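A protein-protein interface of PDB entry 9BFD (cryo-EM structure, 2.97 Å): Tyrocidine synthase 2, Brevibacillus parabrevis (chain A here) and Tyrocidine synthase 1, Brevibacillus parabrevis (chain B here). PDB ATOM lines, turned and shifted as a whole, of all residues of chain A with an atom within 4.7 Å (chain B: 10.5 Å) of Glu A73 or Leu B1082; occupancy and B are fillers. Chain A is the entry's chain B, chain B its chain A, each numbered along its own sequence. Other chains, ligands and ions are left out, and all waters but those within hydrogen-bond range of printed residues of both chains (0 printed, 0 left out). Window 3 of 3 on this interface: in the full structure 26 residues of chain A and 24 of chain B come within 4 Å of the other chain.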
ATOM      1  N   LEU A  71       7.982   6.483 -14.710  1.00  0.00           N
ATOM      2  CA  LEU A  71       9.039   5.494 -14.568  1.00  0.00           C
ATOM      3  C   LEU A  71      10.075   5.721 -15.655  1.00  0.00           C
ATOM      4  O   LEU A  71       9.762   5.627 -16.846  1.00  0.00           O
ATOM      5  CB  LEU A  71       8.470   4.078 -14.650  1.00  0.00           C
ATOM      6  CG  LEU A  71       9.161   3.034 -13.786  1.00  0.00           C
ATOM      7  CD1 LEU A  71       8.847   3.297 -12.331  1.00  0.00           C
ATOM      8  CD2 LEU A  71       8.722   1.643 -14.186  1.00  0.00           C
ATOM      9  N   TYR A  72      11.301   6.024 -15.242  1.00  0.00           N
ATOM     10  CA  TYR A  72      12.375   6.381 -16.154  1.00  0.00           C
ATOM     11  C   TYR A  72      13.662   5.610 -15.912  1.00  0.00           C
ATOM     12  O   TYR A  72      14.634   5.826 -16.642  1.00  0.00           O
ATOM     13  CB  TYR A  72      12.660   7.886 -16.063  1.00  0.00           C
ATOM     14  CG  TYR A  72      12.953   8.350 -14.658  1.00  0.00           C
ATOM     15  CD1 TYR A  72      14.211   8.192 -14.096  1.00  0.00           C
ATOM     16  CD2 TYR A  72      11.953   8.910 -13.873  1.00  0.00           C
ATOM     17  CE1 TYR A  72      14.482   8.641 -12.821  1.00  0.00           C
ATOM     18  CE2 TYR A  72      12.204   9.329 -12.584  1.00  0.00           C
ATOM     19  CZ  TYR A  72      13.473   9.200 -12.064  1.00  0.00           C
ATOM     20  OH  TYR A  72      13.721   9.585 -10.767  1.00  0.00           O
ATOM     21  N   GLU A  73      13.704   4.725 -14.915  1.00  0.00           N
ATOM     22  CA  GLU A  73      14.981   4.317 -14.342  1.00  0.00           C
ATOM     23  C   GLU A  73      15.824   3.543 -15.347  1.00  0.00           C
ATOM     24  O   GLU A  73      16.903   3.994 -15.747  1.00  0.00           O
ATOM     25  CB  GLU A  73      14.744   3.487 -13.081  1.00  0.00           C
ATOM     26  CG  GLU A  73      14.169   4.280 -11.921  1.00  0.00           C
ATOM     27  CD  GLU A  73      15.204   5.160 -11.245  1.00  0.00           C
ATOM     28  OE1 GLU A  73      16.396   5.066 -11.609  1.00  0.00           O
ATOM     29  OE2 GLU A  73      14.827   5.942 -10.348  1.00  0.00           O
ATOM     30  N   LYS A  74      15.344   2.383 -15.786  1.00  0.00           N
ATOM     31  CA  LYS A  74      16.118   1.539 -16.685  1.00  0.00           C
ATOM     32  C   LYS A  74      15.421   1.314 -18.017  1.00  0.00           C
ATOM     33  O   LYS A  74      15.915   0.538 -18.843  1.00  0.00           O
ATOM     34  CB  LYS A  74      16.426   0.198 -16.019  1.00  0.00           C
ATOM     35  CG  LYS A  74      17.246   0.321 -14.753  1.00  0.00           C
ATOM     36  CD  LYS A  74      17.668  -1.040 -14.243  1.00  0.00           C
ATOM     37  CE  LYS A  74      18.073  -0.977 -12.782  1.00  0.00           C
ATOM     38  NZ  LYS A  74      19.199  -0.029 -12.561  1.00  0.00           N
ATOM     39  N   LEU A  75      14.291   1.970 -18.247  1.00  0.00           N
ATOM     40  CA  LEU A  75      13.459   1.671 -19.396  1.00  0.00           C
ATOM     41  C   LEU A  75      14.043   2.298 -20.658  1.00  0.00           C
ATOM     42  O   LEU A  75      14.817   3.257 -20.608  1.00  0.00           O
ATOM     43  CB  LEU A  75      12.035   2.170 -19.160  1.00  0.00           C
ATOM     44  CG  LEU A  75      11.154   1.328 -18.233  1.00  0.00           C
ATOM     45  CD1 LEU A  75      11.778   1.180 -16.858  1.00  0.00           C
ATOM     46  CD2 LEU A  75       9.772   1.942 -18.128  1.00  0.00           C
ATOM     47  N   SER A1015      19.369   6.387 -18.483  1.00  0.00           N
ATOM     48  CA  SER A1015      18.663   5.153 -18.143  1.00  0.00           C
ATOM     49  C   SER A1015      19.295   3.935 -18.807  1.00  0.00           C
ATOM     50  O   SER A1015      19.435   2.873 -18.174  1.00  0.00           O
ATOM     51  CB  SER A1015      17.192   5.265 -18.539  1.00  0.00           C
ATOM     52  OG  SER A1015      17.057   5.572 -19.917  1.00  0.00           O
ATOM     53  N   GLN A1018      22.589   3.294 -16.749  1.00  0.00           N
ATOM     54  CA  GLN A1018      22.229   2.724 -15.457  1.00  0.00           C
ATOM     55  C   GLN A1018      21.498   1.397 -15.579  1.00  0.00           C
ATOM     56  O   GLN A1018      21.102   0.832 -14.556  1.00  0.00           O
ATOM     57  CB  GLN A1018      21.397   3.717 -14.641  1.00  0.00           C
ATOM     58  CG  GLN A1018      19.985   3.944 -15.126  1.00  0.00           C
ATOM     59  CD  GLN A1018      19.010   4.079 -13.974  1.00  0.00           C
ATOM     60  OE1 GLN A1018      18.742   3.117 -13.255  1.00  0.00           O
ATOM     61  NE2 GLN A1018      18.476   5.282 -13.789  1.00  0.00           N
ATOM     62  N   GLU B1074       9.748  -8.738 -23.272  1.00  0.00           N
ATOM     63  CA  GLU B1074      10.912  -8.491 -22.428  1.00  0.00           C
ATOM     64  C   GLU B1074      10.831  -7.129 -21.758  1.00  0.00           C
ATOM     65  O   GLU B1074      11.075  -7.006 -20.551  1.00  0.00           O
ATOM     66  CB  GLU B1074      12.190  -8.605 -23.256  1.00  0.00           C
ATOM     67  CG  GLU B1074      13.469  -8.488 -22.443  1.00  0.00           C
ATOM     68  CD  GLU B1074      13.796  -9.761 -21.689  1.00  0.00           C
ATOM     69  OE1 GLU B1074      12.930 -10.659 -21.632  1.00  0.00           O
ATOM     70  OE2 GLU B1074      14.920  -9.864 -21.154  1.00  0.00           O
ATOM     71  N   GLU B1075      10.361  -6.118 -22.489  1.00  0.00           N
ATOM     72  CA  GLU B1075      10.240  -4.790 -21.902  1.00  0.00           C
ATOM     73  C   GLU B1075       9.069  -4.716 -20.936  1.00  0.00           C
ATOM     74  O   GLU B1075       9.169  -4.073 -19.887  1.00  0.00           O
ATOM     75  CB  GLU B1075      10.099  -3.739 -23.001  1.00  0.00           C
ATOM     76  CG  GLU B1075      10.358  -2.320 -22.527  1.00  0.00           C
ATOM     77  CD  GLU B1075      11.829  -2.048 -22.276  1.00  0.00           C
ATOM     78  OE1 GLU B1075      12.672  -2.828 -22.766  1.00  0.00           O
ATOM     79  OE2 GLU B1075      12.142  -1.054 -21.587  1.00  0.00           O
ATOM     80  N   MET B1076       7.945  -5.345 -21.271  1.00  0.00           N
ATOM     81  CA  MET B1076       6.794  -5.297 -20.379  1.00  0.00           C
ATOM     82  C   MET B1076       7.111  -5.953 -19.040  1.00  0.00           C
ATOM     83  O   MET B1076       6.854  -5.376 -17.975  1.00  0.00           O
ATOM     84  CB  MET B1076       5.588  -5.968 -21.033  1.00  0.00           C
ATOM     85  CG  MET B1076       4.298  -5.778 -20.259  1.00  0.00           C
ATOM     86  SD  MET B1076       2.979  -6.887 -20.765  1.00  0.00           S
ATOM     87  CE  MET B1076       3.549  -8.427 -20.064  1.00  0.00           C
ATOM     88  N   ASP B1077       7.665  -7.168 -19.069  1.00  0.00           N
ATOM     89  CA  ASP B1077       8.033  -7.823 -17.820  1.00  0.00           C
ATOM     90  C   ASP B1077       9.221  -7.173 -17.115  1.00  0.00           C
ATOM     91  O   ASP B1077       9.286  -7.226 -15.881  1.00  0.00           O
ATOM     92  CB  ASP B1077       8.335  -9.296 -18.078  1.00  0.00           C
ATOM     93  CG  ASP B1077       7.079 -10.126 -18.245  1.00  0.00           C
ATOM     94  OD1 ASP B1077       6.030  -9.737 -17.688  1.00  0.00           O
ATOM     95  OD2 ASP B1077       7.138 -11.165 -18.933  1.00  0.00           O
ATOM     96  N   ASP B1078      10.089  -6.451 -17.829  1.00  0.00           N
ATOM     97  CA  ASP B1078      11.104  -5.670 -17.131  1.00  0.00           C
ATOM     98  C   ASP B1078      10.492  -4.470 -16.421  1.00  0.00           C
ATOM     99  O   ASP B1078      10.865  -4.155 -15.284  1.00  0.00           O
ATOM    100  CB  ASP B1078      12.186  -5.223 -18.112  1.00  0.00           C
ATOM    101  CG  ASP B1078      13.387  -4.617 -17.417  1.00  0.00           C
ATOM    102  OD1 ASP B1078      13.681  -5.024 -16.273  1.00  0.00           O
ATOM    103  OD2 ASP B1078      14.039  -3.733 -18.012  1.00  0.00           O
ATOM    104  N   ILE B1079       9.540  -3.800 -17.065  1.00  0.00           N
ATOM    105  CA  ILE B1079       8.826  -2.708 -16.411  1.00  0.00           C
ATOM    106  C   ILE B1079       8.116  -3.215 -15.167  1.00  0.00           C
ATOM    107  O   ILE B1079       8.179  -2.594 -14.099  1.00  0.00           O
ATOM    108  CB  ILE B1079       7.842  -2.048 -17.392  1.00  0.00           C
ATOM    109  CG1 ILE B1079       8.597  -1.212 -18.426  1.00  0.00           C
ATOM    110  CG2 ILE B1079       6.837  -1.197 -16.646  1.00  0.00           C
ATOM    111  CD1 ILE B1079       7.820  -0.966 -19.699  1.00  0.00           C
ATOM    112  N   PHE B1080       7.409  -4.339 -15.287  1.00  0.00           N
ATOM    113  CA  PHE B1080       6.700  -4.858 -14.123  1.00  0.00           C
ATOM    114  C   PHE B1080       7.652  -5.266 -13.009  1.00  0.00           C
ATOM    115  O   PHE B1080       7.319  -5.113 -11.829  1.00  0.00           O
ATOM    116  CB  PHE B1080       5.820  -6.038 -14.518  1.00  0.00           C
ATOM    117  CG  PHE B1080       4.508  -5.638 -15.108  1.00  0.00           C
ATOM    118  CD1 PHE B1080       3.540  -5.046 -14.325  1.00  0.00           C
ATOM    119  CD2 PHE B1080       4.241  -5.853 -16.443  1.00  0.00           C
ATOM    120  CE1 PHE B1080       2.333  -4.678 -14.862  1.00  0.00           C
ATOM    121  CE2 PHE B1080       3.034  -5.487 -16.984  1.00  0.00           C
ATOM    122  CZ  PHE B1080       2.080  -4.899 -16.192  1.00  0.00           C
ATOM    123  N   GLU B1081       8.833  -5.788 -13.346  1.00  0.00           N
ATOM    124  CA  GLU B1081       9.822  -6.053 -12.306  1.00  0.00           C
ATOM    125  C   GLU B1081      10.283  -4.763 -11.640  1.00  0.00           C
ATOM    126  O   GLU B1081      10.490  -4.721 -10.422  1.00  0.00           O
ATOM    127  CB  GLU B1081      11.012  -6.814 -12.886  1.00  0.00           C
ATOM    128  CG  GLU B1081      11.984  -7.315 -11.838  1.00  0.00           C
ATOM    129  CD  GLU B1081      13.027  -8.250 -12.411  1.00  0.00           C
ATOM    130  OE1 GLU B1081      12.646  -9.204 -13.124  1.00  0.00           O
ATOM    131  OE2 GLU B1081      14.229  -8.033 -12.151  1.00  0.00           O
ATOM    132  N   LEU B1082      10.448  -3.700 -12.427  1.00  0.00           N
ATOM    133  CA  LEU B1082      10.883  -2.421 -11.876  1.00  0.00           C
ATOM    134  C   LEU B1082       9.826  -1.771 -10.992  1.00  0.00           C
ATOM    135  O   LEU B1082      10.172  -1.061 -10.043  1.00  0.00           O
ATOM    136  CB  LEU B1082      11.272  -1.475 -13.009  1.00  0.00           C
ATOM    137  CG  LEU B1082      12.220  -0.336 -12.648  1.00  0.00           C
ATOM    138  CD1 LEU B1082      13.265  -0.155 -13.736  1.00  0.00           C
ATOM    139  CD2 LEU B1082      11.445   0.950 -12.429  1.00  0.00           C
ATOM    140  N   LEU B1083       8.543  -1.993 -11.279  1.00  0.00           N
ATOM    141  CA  LEU B1083       7.503  -1.552 -10.353  1.00  0.00           C
ATOM    142  C   LEU B1083       7.600  -2.267  -9.012  1.00  0.00           C
ATOM    143  O   LEU B1083       7.473  -1.638  -7.956  1.00  0.00           O
ATOM    144  CB  LEU B1083       6.121  -1.758 -10.969  1.00  0.00           C
ATOM    145  CG  LEU B1083       5.730  -0.787 -12.081  1.00  0.00           C
ATOM    146  CD1 LEU B1083       4.527  -1.298 -12.846  1.00  0.00           C
ATOM    147  CD2 LEU B1083       5.449   0.583 -11.504  1.00  0.00           C
ATOM    148  N   ALA B1084       7.821  -3.580  -9.029  1.00  0.00           N
ATOM    149  CA  ALA B1084       7.975  -4.310  -7.777  1.00  0.00           C
ATOM    150  C   ALA B1084       9.185  -3.837  -6.982  1.00  0.00           C
ATOM    151  O   ALA B1084       9.155  -3.846  -5.747  1.00  0.00           O
ATOM    152  CB  ALA B1084       8.076  -5.810  -8.052  1.00  0.00           C
ATOM    153  N   ASN B1085      10.250  -3.418  -7.660  1.00  0.00           N
ATOM    154  CA  ASN B1085      11.402  -2.825  -6.993  1.00  0.00           C
ATOM    155  C   ASN B1085      11.229  -1.340  -6.702  1.00  0.00           C
ATOM    156  O   ASN B1085      12.213  -0.674  -6.369  1.00  0.00           O
ATOM    157  CB  ASN B1085      12.663  -3.041  -7.830  1.00  0.00           C
ATOM    158  CG  ASN B1085      13.088  -4.492  -7.875  1.00  0.00           C
ATOM    159  OD1 ASN B1085      12.807  -5.263  -6.957  1.00  0.00           O
ATOM    160  ND2 ASN B1085      13.775  -4.876  -8.945  1.00  0.00           N
ATOM    161  N   ARG B1086      10.012  -0.801  -6.826  1.00  0.00           N
ATOM    162  CA  ARG B1086       9.816   0.622  -6.573  1.00  0.00           C
ATOM    163  C   ARG B1086       8.460   0.921  -5.942  1.00  0.00           C
ATOM    164  O   ARG B1086       7.987   2.058  -6.044  1.00  0.00           O
ATOM    165  CB  ARG B1086       9.962   1.430  -7.869  1.00  0.00           C
ATOM    166  N   LEU B1087       7.818  -0.054  -5.310  1.00  0.00           N
ATOM    167  CA  LEU B1087       6.583   0.188  -4.579  1.00  0.00           C
ATOM    168  C   LEU B1087       6.536  -0.670  -3.320  1.00  0.00           C
ATOM    169  O   LEU B1087       5.570  -0.631  -2.561  1.00  0.00           O
ATOM    170  CB  LEU B1087       5.364  -0.088  -5.459  1.00  0.00           C
ATOM    171  CG  LEU B1087       5.146   0.863  -6.639  1.00  0.00           C
ATOM    172  CD1 LEU B1087       4.019   0.366  -7.523  1.00  0.00           C
ATOM    173  CD2 LEU B1087       4.862   2.272  -6.150  1.00  0.00           C
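The side-chain hydroxyl (OG) of Ser A1015 is in hydrogen-bond range of the backbone carbonyl oxygen (O) of Leu A75, at 3.3 Å.
The side-chain amino group (NZ) of Lys A74 is in hydrogen-bond range of the backbone carbonyl oxygen (O) of Gln A1018.
The side-chain amide nitrogen of Gln A1018 lies close to the backbone carbonyl oxygen of Glu A73 (2.8 Å).
Printed residues of chain A that touch a printed residue of chain B: Leu A71, Glu A73, Lys A74 and Leu A75.
Hydrophobic or aromatic side chains of chain A that line the printed part of chain B: Leu A71 and Leu A75.
Of the 14 printed residues of chain B, 3 touch a printed residue of chain A.
Hydrophobic or aromatic side chains of chain B that line the printed part of chain A: Ile B1079 and Leu B1082.
Among the printed residues, no Asp or Glu carboxylate lies within 4 Å of a Lys or Arg side-chain nitrogen of the other chain.
CD2 of Leu A71 touches CD2 of Leu B1082 (3.3 Å).
Leu B1082 touches Glu A73.
Lys A74 touches Leu B1082 (N to CD1, 3.9 Å).
OE2 of Glu B1075 touches CA of Leu A75, 3.7 Å away.
Leu A75 touches Ile B1079 (CD2 to CG1, 3.4 Å).
Leu A75 touches Leu B1082.
Leu A71 touches just one residue of chain B: Leu B1082.
No residue of chain B comes within 4 Å of Tyr A72.
Of the printed residues of chain B, Glu A73 touches Leu B1082.
Printed residues of chain B within 4 Å of Lys A74: Leu B1082 (3.9 Å).
Leu A75 touches just these residues of chain B: Glu B1075 (3.7 Å), Ile B1079 (3.4 Å) and Leu B1082 (3.7 Å).
No residue of chain B comes within 4 Å of Ser A1015.
No residue of chain B comes within 4 Å of Gln A1018.
Printed residues of chain A within 4 Å of Glu B1075: Leu A75 (3.7 Å).
Of the printed residues of chain A, Ile B1079 touches Leu A75.
Of the printed residues of chain A, Leu B1082 touches Leu A71 (3.3 Å), Glu A73 (3.99 Å), Lys A74 (3.9 Å) and Leu A75 (3.7 Å).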
